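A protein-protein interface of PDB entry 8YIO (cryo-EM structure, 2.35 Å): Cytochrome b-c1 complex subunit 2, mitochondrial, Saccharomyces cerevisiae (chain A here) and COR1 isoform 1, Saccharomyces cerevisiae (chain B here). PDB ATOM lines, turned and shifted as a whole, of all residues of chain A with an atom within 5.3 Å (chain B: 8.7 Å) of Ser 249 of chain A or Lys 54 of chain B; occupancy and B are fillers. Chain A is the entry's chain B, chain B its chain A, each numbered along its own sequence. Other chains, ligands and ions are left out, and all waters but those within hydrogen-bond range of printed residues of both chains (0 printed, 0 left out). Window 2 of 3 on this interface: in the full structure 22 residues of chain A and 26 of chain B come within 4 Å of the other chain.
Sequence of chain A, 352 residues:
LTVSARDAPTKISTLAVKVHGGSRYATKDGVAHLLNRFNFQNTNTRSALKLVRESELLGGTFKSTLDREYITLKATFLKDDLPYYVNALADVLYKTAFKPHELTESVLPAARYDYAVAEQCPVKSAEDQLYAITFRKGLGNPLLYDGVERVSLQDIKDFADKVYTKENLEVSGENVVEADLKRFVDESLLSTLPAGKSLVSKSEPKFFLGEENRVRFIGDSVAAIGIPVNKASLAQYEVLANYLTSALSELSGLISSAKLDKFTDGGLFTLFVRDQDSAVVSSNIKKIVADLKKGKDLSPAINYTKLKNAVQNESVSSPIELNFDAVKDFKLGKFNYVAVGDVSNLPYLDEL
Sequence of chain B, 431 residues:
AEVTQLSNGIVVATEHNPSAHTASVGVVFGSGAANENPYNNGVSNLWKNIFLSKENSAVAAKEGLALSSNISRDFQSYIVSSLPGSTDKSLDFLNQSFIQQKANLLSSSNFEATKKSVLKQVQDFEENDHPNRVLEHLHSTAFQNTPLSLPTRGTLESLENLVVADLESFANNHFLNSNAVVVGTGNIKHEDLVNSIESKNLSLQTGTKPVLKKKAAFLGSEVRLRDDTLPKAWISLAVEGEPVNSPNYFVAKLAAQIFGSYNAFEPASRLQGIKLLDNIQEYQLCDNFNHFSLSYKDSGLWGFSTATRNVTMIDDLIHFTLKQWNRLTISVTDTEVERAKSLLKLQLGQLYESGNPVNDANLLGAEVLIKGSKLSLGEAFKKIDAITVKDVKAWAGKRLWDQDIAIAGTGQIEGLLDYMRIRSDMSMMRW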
ATOM      1  N   TYR A 243      -6.704  19.998  21.323  1.00  0.00           N
ATOM      2  CA  TYR A 243      -7.212  20.536  22.580  1.00  0.00           C
ATOM      3  C   TYR A 243      -7.615  21.998  22.437  1.00  0.00           C
ATOM      4  O   TYR A 243      -8.626  22.423  23.002  1.00  0.00           O
ATOM      5  CB  TYR A 243      -6.157  20.368  23.674  1.00  0.00           C
ATOM      6  CG  TYR A 243      -6.356  21.209  24.915  1.00  0.00           C
ATOM      7  CD1 TYR A 243      -7.289  20.849  25.878  1.00  0.00           C
ATOM      8  CD2 TYR A 243      -5.585  22.343  25.140  1.00  0.00           C
ATOM      9  CE1 TYR A 243      -7.465  21.608  27.018  1.00  0.00           C
ATOM     10  CE2 TYR A 243      -5.755  23.108  26.272  1.00  0.00           C
ATOM     11  CZ  TYR A 243      -6.695  22.735  27.210  1.00  0.00           C
ATOM     12  OH  TYR A 243      -6.864  23.494  28.340  1.00  0.00           O
ATOM     13  N   LEU A 244      -6.847  22.775  21.673  1.00  0.00           N
ATOM     14  CA  LEU A 244      -7.084  24.209  21.574  1.00  0.00           C
ATOM     15  C   LEU A 244      -8.327  24.554  20.762  1.00  0.00           C
ATOM     16  O   LEU A 244      -8.896  25.629  20.963  1.00  0.00           O
ATOM     17  CB  LEU A 244      -5.864  24.904  20.968  1.00  0.00           C
ATOM     18  CG  LEU A 244      -4.663  25.131  21.889  1.00  0.00           C
ATOM     19  CD1 LEU A 244      -3.498  25.723  21.118  1.00  0.00           C
ATOM     20  CD2 LEU A 244      -5.030  26.010  23.071  1.00  0.00           C
ATOM     21  N   SER A 246     -11.169  22.588  20.633  1.00  0.00           N
ATOM     22  CA  SER A 246     -12.303  21.819  21.120  1.00  0.00           C
ATOM     23  C   SER A 246     -12.986  22.564  22.263  1.00  0.00           C
ATOM     24  O   SER A 246     -12.551  23.635  22.692  1.00  0.00           O
ATOM     25  CB  SER A 246     -11.863  20.425  21.568  1.00  0.00           C
ATOM     26  OG  SER A 246     -11.010  20.493  22.691  1.00  0.00           O
ATOM     27  N   ALA A 247     -14.062  21.967  22.773  1.00  0.00           N
ATOM     28  CA  ALA A 247     -14.810  22.540  23.883  1.00  0.00           C
ATOM     29  C   ALA A 247     -14.135  22.335  25.233  1.00  0.00           C
ATOM     30  O   ALA A 247     -14.626  22.863  26.236  1.00  0.00           O
ATOM     31  CB  ALA A 247     -16.219  21.948  23.920  1.00  0.00           C
ATOM     32  N   LEU A 248     -13.030  21.589  25.289  1.00  0.00           N
ATOM     33  CA  LEU A 248     -12.306  21.402  26.539  1.00  0.00           C
ATOM     34  C   LEU A 248     -11.484  22.623  26.928  1.00  0.00           C
ATOM     35  O   LEU A 248     -11.073  22.732  28.086  1.00  0.00           O
ATOM     36  CB  LEU A 248     -11.388  20.184  26.439  1.00  0.00           C
ATOM     37  CG  LEU A 248     -12.054  18.855  26.095  1.00  0.00           C
ATOM     38  CD1 LEU A 248     -11.025  17.832  25.667  1.00  0.00           C
ATOM     39  CD2 LEU A 248     -12.843  18.354  27.281  1.00  0.00           C
ATOM     40  N   SER A 249     -11.231  23.532  25.992  1.00  0.00           N
ATOM     41  CA  SER A 249     -10.406  24.706  26.226  1.00  0.00           C
ATOM     42  C   SER A 249     -11.262  25.963  26.213  1.00  0.00           C
ATOM     43  O   SER A 249     -12.125  26.129  25.346  1.00  0.00           O
ATOM     44  CB  SER A 249      -9.308  24.824  25.168  1.00  0.00           C
ATOM     45  OG  SER A 249      -8.613  26.050  25.289  1.00  0.00           O
ATOM     46  N   GLU A 250     -11.013  26.850  27.175  1.00  0.00           N
ATOM     47  CA  GLU A 250     -11.700  28.132  27.234  1.00  0.00           C
ATOM     48  C   GLU A 250     -11.191  29.131  26.202  1.00  0.00           C
ATOM     49  O   GLU A 250     -11.852  30.149  25.974  1.00  0.00           O
ATOM     50  CB  GLU A 250     -11.570  28.732  28.636  1.00  0.00           C
ATOM     51  CG  GLU A 250     -10.162  29.188  28.998  1.00  0.00           C
ATOM     52  CD  GLU A 250      -9.319  28.096  29.638  1.00  0.00           C
ATOM     53  OE1 GLU A 250      -9.705  26.910  29.577  1.00  0.00           O
ATOM     54  OE2 GLU A 250      -8.256  28.430  30.200  1.00  0.00           O
ATOM     55  N   LEU A 251     -10.047  28.867  25.574  1.00  0.00           N
ATOM     56  CA  LEU A 251      -9.473  29.750  24.568  1.00  0.00           C
ATOM     57  C   LEU A 251      -9.986  29.481  23.161  1.00  0.00           C
ATOM     58  O   LEU A 251      -9.553  30.162  22.228  1.00  0.00           O
ATOM     59  CB  LEU A 251      -7.946  29.625  24.563  1.00  0.00           C
ATOM     60  CG  LEU A 251      -7.163  29.930  25.839  1.00  0.00           C
ATOM     61  CD1 LEU A 251      -5.717  29.501  25.670  1.00  0.00           C
ATOM     62  CD2 LEU A 251      -7.252  31.401  26.206  1.00  0.00           C
ATOM     63  N   SER A 252     -10.882  28.506  22.979  1.00  0.00           N
ATOM     64  CA  SER A 252     -11.259  28.085  21.633  1.00  0.00           C
ATOM     65  C   SER A 252     -12.144  29.097  20.921  1.00  0.00           C
ATOM     66  O   SER A 252     -12.207  29.080  19.689  1.00  0.00           O
ATOM     67  CB  SER A 252     -11.961  26.727  21.677  1.00  0.00           C
ATOM     68  OG  SER A 252     -13.053  26.736  22.573  1.00  0.00           O
ATOM     69  N   LYS A 296      -0.242  24.285  30.476  1.00  0.00           N
ATOM     70  CA  LYS A 296      -1.514  23.591  30.361  1.00  0.00           C
ATOM     71  C   LYS A 296      -1.318  22.108  30.635  1.00  0.00           C
ATOM     72  O   LYS A 296      -0.237  21.558  30.413  1.00  0.00           O
ATOM     73  CB  LYS A 296      -2.135  23.772  28.971  1.00  0.00           C
ATOM     74  CG  LYS A 296      -2.661  25.163  28.694  1.00  0.00           C
ATOM     75  CD  LYS A 296      -3.908  25.453  29.502  1.00  0.00           C
ATOM     76  CE  LYS A 296      -4.325  26.901  29.349  1.00  0.00           C
ATOM     77  NZ  LYS A 296      -4.302  27.303  27.923  1.00  0.00           N
ATOM     78  N   ASN B  49     -28.131  23.748  17.010  1.00  0.00           N
ATOM     79  CA  ASN B  49     -27.075  24.457  17.715  1.00  0.00           C
ATOM     80  C   ASN B  49     -27.191  24.342  19.230  1.00  0.00           C
ATOM     81  O   ASN B  49     -26.219  24.631  19.930  1.00  0.00           O
ATOM     82  CB  ASN B  49     -27.068  25.924  17.290  1.00  0.00           C
ATOM     83  CG  ASN B  49     -26.567  26.112  15.875  1.00  0.00           C
ATOM     84  OD1 ASN B  49     -25.383  26.342  15.653  1.00  0.00           O
ATOM     85  ND2 ASN B  49     -27.467  26.008  14.908  1.00  0.00           N
ATOM     86  N   ILE B  50     -28.348  23.927  19.746  1.00  0.00           N
ATOM     87  CA  ILE B  50     -28.449  23.565  21.156  1.00  0.00           C
ATOM     88  C   ILE B  50     -27.715  22.253  21.411  1.00  0.00           C
ATOM     89  O   ILE B  50     -26.988  22.110  22.403  1.00  0.00           O
ATOM     90  CB  ILE B  50     -29.935  23.495  21.571  1.00  0.00           C
ATOM     91  CG1 ILE B  50     -30.512  24.902  21.755  1.00  0.00           C
ATOM     92  CG2 ILE B  50     -30.145  22.674  22.835  1.00  0.00           C
ATOM     93  CD1 ILE B  50     -29.922  25.670  22.910  1.00  0.00           C
ATOM     94  N   PHE B  51     -27.863  21.291  20.496  1.00  0.00           N
ATOM     95  CA  PHE B  51     -27.188  20.001  20.607  1.00  0.00           C
ATOM     96  C   PHE B  51     -25.680  20.134  20.425  1.00  0.00           C
ATOM     97  O   PHE B  51     -24.917  19.369  21.023  1.00  0.00           O
ATOM     98  CB  PHE B  51     -27.789  19.034  19.581  1.00  0.00           C
ATOM     99  CG  PHE B  51     -27.142  17.677  19.547  1.00  0.00           C
ATOM    100  CD1 PHE B  51     -27.357  16.763  20.565  1.00  0.00           C
ATOM    101  CD2 PHE B  51     -26.342  17.306  18.477  1.00  0.00           C
ATOM    102  CE1 PHE B  51     -26.768  15.509  20.526  1.00  0.00           C
ATOM    103  CE2 PHE B  51     -25.753  16.055  18.433  1.00  0.00           C
ATOM    104  CZ  PHE B  51     -25.969  15.158  19.457  1.00  0.00           C
ATOM    105  N   LEU B  52     -25.232  21.103  19.628  1.00  0.00           N
ATOM    106  CA  LEU B  52     -23.816  21.321  19.373  1.00  0.00           C
ATOM    107  C   LEU B  52     -23.222  22.431  20.240  1.00  0.00           C
ATOM    108  O   LEU B  52     -22.153  22.955  19.911  1.00  0.00           O
ATOM    109  CB  LEU B  52     -23.589  21.634  17.892  1.00  0.00           C
ATOM    110  CG  LEU B  52     -23.916  20.557  16.851  1.00  0.00           C
ATOM    111  CD1 LEU B  52     -23.770  21.108  15.444  1.00  0.00           C
ATOM    112  CD2 LEU B  52     -23.050  19.326  17.030  1.00  0.00           C
ATOM    113  N   SER B  53     -23.881  22.793  21.340  1.00  0.00           N
ATOM    114  CA  SER B  53     -23.397  23.861  22.202  1.00  0.00           C
ATOM    115  C   SER B  53     -22.190  23.394  23.019  1.00  0.00           C
ATOM    116  O   SER B  53     -21.834  22.215  23.035  1.00  0.00           O
ATOM    117  CB  SER B  53     -24.509  24.357  23.124  1.00  0.00           C
ATOM    118  OG  SER B  53     -25.211  23.279  23.711  1.00  0.00           O
ATOM    119  N   LYS B  54     -21.570  24.350  23.717  1.00  0.00           N
ATOM    120  CA  LYS B  54     -20.221  24.147  24.240  1.00  0.00           C
ATOM    121  C   LYS B  54     -20.202  23.205  25.439  1.00  0.00           C
ATOM    122  O   LYS B  54     -19.305  22.362  25.555  1.00  0.00           O
ATOM    123  CB  LYS B  54     -19.600  25.496  24.601  1.00  0.00           C
ATOM    124  CG  LYS B  54     -18.157  25.401  25.060  1.00  0.00           C
ATOM    125  CD  LYS B  54     -17.525  26.760  25.270  1.00  0.00           C
ATOM    126  CE  LYS B  54     -16.157  26.614  25.915  1.00  0.00           C
ATOM    127  NZ  LYS B  54     -15.190  25.912  25.030  1.00  0.00           N
ATOM    128  N   GLU B  55     -21.185  23.323  26.333  1.00  0.00           N
ATOM    129  CA  GLU B  55     -21.229  22.464  27.512  1.00  0.00           C
ATOM    130  C   GLU B  55     -21.623  21.038  27.149  1.00  0.00           C
ATOM    131  O   GLU B  55     -21.170  20.085  27.793  1.00  0.00           O
ATOM    132  CB  GLU B  55     -22.207  23.048  28.533  1.00  0.00           C
ATOM    133  CG  GLU B  55     -22.309  22.380  29.922  1.00  0.00           C
ATOM    134  CD  GLU B  55     -21.043  22.404  30.759  1.00  0.00           C
ATOM    135  OE1 GLU B  55     -20.035  21.745  30.421  1.00  0.00           O
ATOM    136  OE2 GLU B  55     -21.040  23.119  31.780  1.00  0.00           O
ATOM    137  N   ASN B  56     -22.453  20.876  26.118  1.00  0.00           N
ATOM    138  CA  ASN B  56     -22.813  19.543  25.651  1.00  0.00           C
ATOM    139  C   ASN B  56     -21.659  18.887  24.906  1.00  0.00           C
ATOM    140  O   ASN B  56     -21.459  17.671  25.008  1.00  0.00           O
ATOM    141  CB  ASN B  56     -24.049  19.625  24.758  1.00  0.00           C
ATOM    142  CG  ASN B  56     -24.845  18.346  24.750  1.00  0.00           C
ATOM    143  OD1 ASN B  56     -24.983  17.685  25.774  1.00  0.00           O
ATOM    144  ND2 ASN B  56     -25.373  17.988  23.591  1.00  0.00           N
ATOM    145  N   SER B  57     -20.893  19.672  24.147  1.00  0.00           N
ATOM    146  CA  SER B  57     -19.739  19.141  23.438  1.00  0.00           C
ATOM    147  C   SER B  57     -18.583  18.814  24.372  1.00  0.00           C
ATOM    148  O   SER B  57     -17.756  17.965  24.034  1.00  0.00           O
ATOM    149  CB  SER B  57     -19.269  20.131  22.373  1.00  0.00           C
ATOM    150  OG  SER B  57     -20.329  20.500  21.515  1.00  0.00           O
ATOM    151  N   ALA B  58     -18.508  19.467  25.532  1.00  0.00           N
ATOM    152  CA  ALA B  58     -17.420  19.214  26.465  1.00  0.00           C
ATOM    153  C   ALA B  58     -17.614  17.918  27.239  1.00  0.00           C
ATOM    154  O   ALA B  58     -16.630  17.250  27.570  1.00  0.00           O
ATOM    155  CB  ALA B  58     -17.274  20.386  27.437  1.00  0.00           C
ATOM    156  N   VAL B  59     -18.864  17.562  27.546  1.00  0.00           N
ATOM    157  CA  VAL B  59     -19.150  16.286  28.196  1.00  0.00           C
ATOM    158  C   VAL B  59     -18.818  15.132  27.258  1.00  0.00           C
ATOM    159  O   VAL B  59     -18.258  14.112  27.678  1.00  0.00           O
ATOM    160  CB  VAL B  59     -20.621  16.261  28.662  1.00  0.00           C
ATOM    161  CG1 VAL B  59     -21.077  14.859  29.052  1.00  0.00           C
ATOM    162  CG2 VAL B  59     -20.820  17.217  29.827  1.00  0.00           C
ATOM    163  N   ALA B  60     -19.097  15.305  25.964  1.00  0.00           N
ATOM    164  CA  ALA B  60     -18.809  14.266  24.984  1.00  0.00           C
ATOM    165  C   ALA B  60     -17.312  14.116  24.745  1.00  0.00           C
ATOM    166  O   ALA B  60     -16.826  13.002  24.522  1.00  0.00           O
ATOM    167  CB  ALA B  60     -19.530  14.573  23.674  1.00  0.00           C
ATOM    168  N   ALA B  61     -16.564  15.221  24.802  1.00  0.00           N
ATOM    169  CA  ALA B  61     -15.146  15.193  24.462  1.00  0.00           C
ATOM    170  C   ALA B  61     -14.293  14.535  25.540  1.00  0.00           C
ATOM    171  O   ALA B  61     -13.238  13.978  25.226  1.00  0.00           O
ATOM    172  CB  ALA B  61     -14.643  16.610  24.191  1.00  0.00           C
ATOM    173  N   LYS B  62     -14.722  14.584  26.805  1.00  0.00           N
ATOM    174  CA  LYS B  62     -14.015  13.859  27.855  1.00  0.00           C
ATOM    175  C   LYS B  62     -14.183  12.350  27.737  1.00  0.00           C
ATOM    176  O   LYS B  62     -13.359  11.606  28.275  1.00  0.00           O
ATOM    177  CB  LYS B  62     -14.479  14.319  29.237  1.00  0.00           C
ATOM    178  CG  LYS B  62     -13.994  15.695  29.622  1.00  0.00           C
ATOM    179  CD  LYS B  62     -14.410  16.065  31.033  1.00  0.00           C
ATOM    180  CE  LYS B  62     -15.879  16.429  31.099  1.00  0.00           C
ATOM    181  NZ  LYS B  62     -16.150  17.690  30.353  1.00  0.00           N
ATOM    182  N   LEU B  67     -19.667  15.129  17.768  1.00  0.00           N
ATOM    183  CA  LEU B  67     -21.082  15.347  17.503  1.00  0.00           C
ATOM    184  C   LEU B  67     -21.288  16.007  16.145  1.00  0.00           C
ATOM    185  O   LEU B  67     -20.494  16.852  15.728  1.00  0.00           O
ATOM    186  CB  LEU B  67     -21.710  16.209  18.601  1.00  0.00           C
ATOM    187  CG  LEU B  67     -21.476  15.767  20.046  1.00  0.00           C
ATOM    188  CD1 LEU B  67     -22.129  16.730  21.022  1.00  0.00           C
ATOM    189  CD2 LEU B  67     -21.983  14.354  20.269  1.00  0.00           C
ATOM    190  N   LEU B 105     -30.025  21.583  28.874  1.00  0.00           N
ATOM    191  CA  LEU B 105     -29.657  22.291  27.657  1.00  0.00           C
ATOM    192  C   LEU B 105     -30.470  23.563  27.462  1.00  0.00           C
ATOM    193  O   LEU B 105     -29.964  24.534  26.892  1.00  0.00           O
ATOM    194  CB  LEU B 105     -29.826  21.371  26.446  1.00  0.00           C
ATOM    195  CG  LEU B 105     -28.819  20.228  26.313  1.00  0.00           C
ATOM    196  CD1 LEU B 105     -29.292  19.208  25.294  1.00  0.00           C
ATOM    197  CD2 LEU B 105     -27.452  20.768  25.936  1.00  0.00           C
ATOM    198  N   ASN B 110     -27.910  29.411  28.551  1.00  0.00           N
ATOM    199  CA  ASN B 110     -27.477  28.706  27.351  1.00  0.00           C
ATOM    200  C   ASN B 110     -28.326  29.060  26.137  1.00  0.00           C
ATOM    201  O   ASN B 110     -27.818  29.050  25.013  1.00  0.00           O
ATOM    202  CB  ASN B 110     -27.512  27.195  27.589  1.00  0.00           C
ATOM    203  CG  ASN B 110     -26.686  26.424  26.578  1.00  0.00           C
ATOM    204  OD1 ASN B 110     -25.617  26.869  26.163  1.00  0.00           O
ATOM    205  ND2 ASN B 110     -27.177  25.260  26.179  1.00  0.00           N
ATOM    206  N   ALA B 113     -27.304  32.690  24.647  1.00  0.00           N
ATOM    207  CA  ALA B 113     -26.017  32.680  23.964  1.00  0.00           C
ATOM    208  C   ALA B 113     -26.086  31.934  22.638  1.00  0.00           C
ATOM    209  O   ALA B 113     -25.391  32.301  21.686  1.00  0.00           O
ATOM    210  CB  ALA B 113     -24.951  32.064  24.867  1.00  0.00           C
ATOM    211  N   THR B 114     -26.916  30.891  22.557  1.00  0.00           N
ATOM    212  CA  THR B 114     -27.058  30.142  21.312  1.00  0.00           C
ATOM    213  C   THR B 114     -27.842  30.940  20.274  1.00  0.00           C
ATOM    214  O   THR B 114     -27.500  30.926  19.087  1.00  0.00           O
ATOM    215  CB  THR B 114     -27.729  28.795  21.595  1.00  0.00           C
ATOM    216  OG1 THR B 114     -26.994  28.103  22.609  1.00  0.00           O
ATOM    217  CG2 THR B 114     -27.772  27.926  20.355  1.00  0.00           C
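Lys 54 of chain B touches three residues of chain A. Printed residues of chain A within 4 Å of Ser 57 of chain B: Ala 247. Printed residues of chain A within 4 Å of Ala 61 of chain B: Leu 248 (3.9 Å). The nearest printed residue of chain B that does not touch Leu 248 of chain A is Lys 54 of chain B (4.8 Å).
NZ of Lys 54 of chain B lies within hydrogen-bond range of O of Ala 247 of chain A, at 3.3 Å. NZ of Lys 54 of chain B is in hydrogen-bond range of OG of Ser 252 of chain A (3.4 Å). O of Ser 249 of chain A lies within hydrogen-bond range of NZ of Lys 54 of chain B, 3.1 Å away.
Of the 19 printed residues of chain B, 5 touch a printed residue of chain A. Hydrophobic or aromatic side chains of chain B that line the printed part of chain A: Ala 58 and Ala 61. Along chain B the printed residues that touch a printed residue of chain A span positions 54 to 62. Of the 10 printed residues of chain A, 4 touch a printed residue of chain B. Hydrophobic or aromatic side chains of chain A that line the printed part of chain B: Ala 247 and Leu 248. Among the printed residues, 8 pairs touch across the chains.
CB of Ser 57 of chain B touches CB of Ala 247 of chain A, 3.9 Å away. Ala 58 of chain B touches Ala 247 of chain A (N to CB, 3.7 Å). Leu 248 of chain A touches Ala 58 of chain B. Ala 61 of chain B touches Leu 248 of chain A (CB to CG, 3.9 Å). CD2 of Leu 248 of chain A touches CG of Lys 62 of chain B (3.7 Å).
O of Leu 52 of chain B sits at hydrogen-bond distance from OG of Ser 57 of chain B (3.5 Å). The backbone carbonyl oxygen of Ala 58 of chain B lies within hydrogen-bond range of the side-chain amino group of Lys 62 of chain B (2.9 Å). OG of Ser 246 of chain A lies close to N of Leu 248 of chain A (3.5 Å). OG of Ser 249 of chain A is in hydrogen-bond range of N of Leu 251 of chain A (3.2 Å). The side-chain hydroxyl of Ser 252 of chain A lies within hydrogen-bond range of the backbone carbonyl oxygen of Ser 246 of chain A. The backbone carbonyl oxygen of Ser 249 of chain A lies within hydrogen-bond range of the side-chain hydroxyl of Ser 252 of chain A (3.0 Å).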
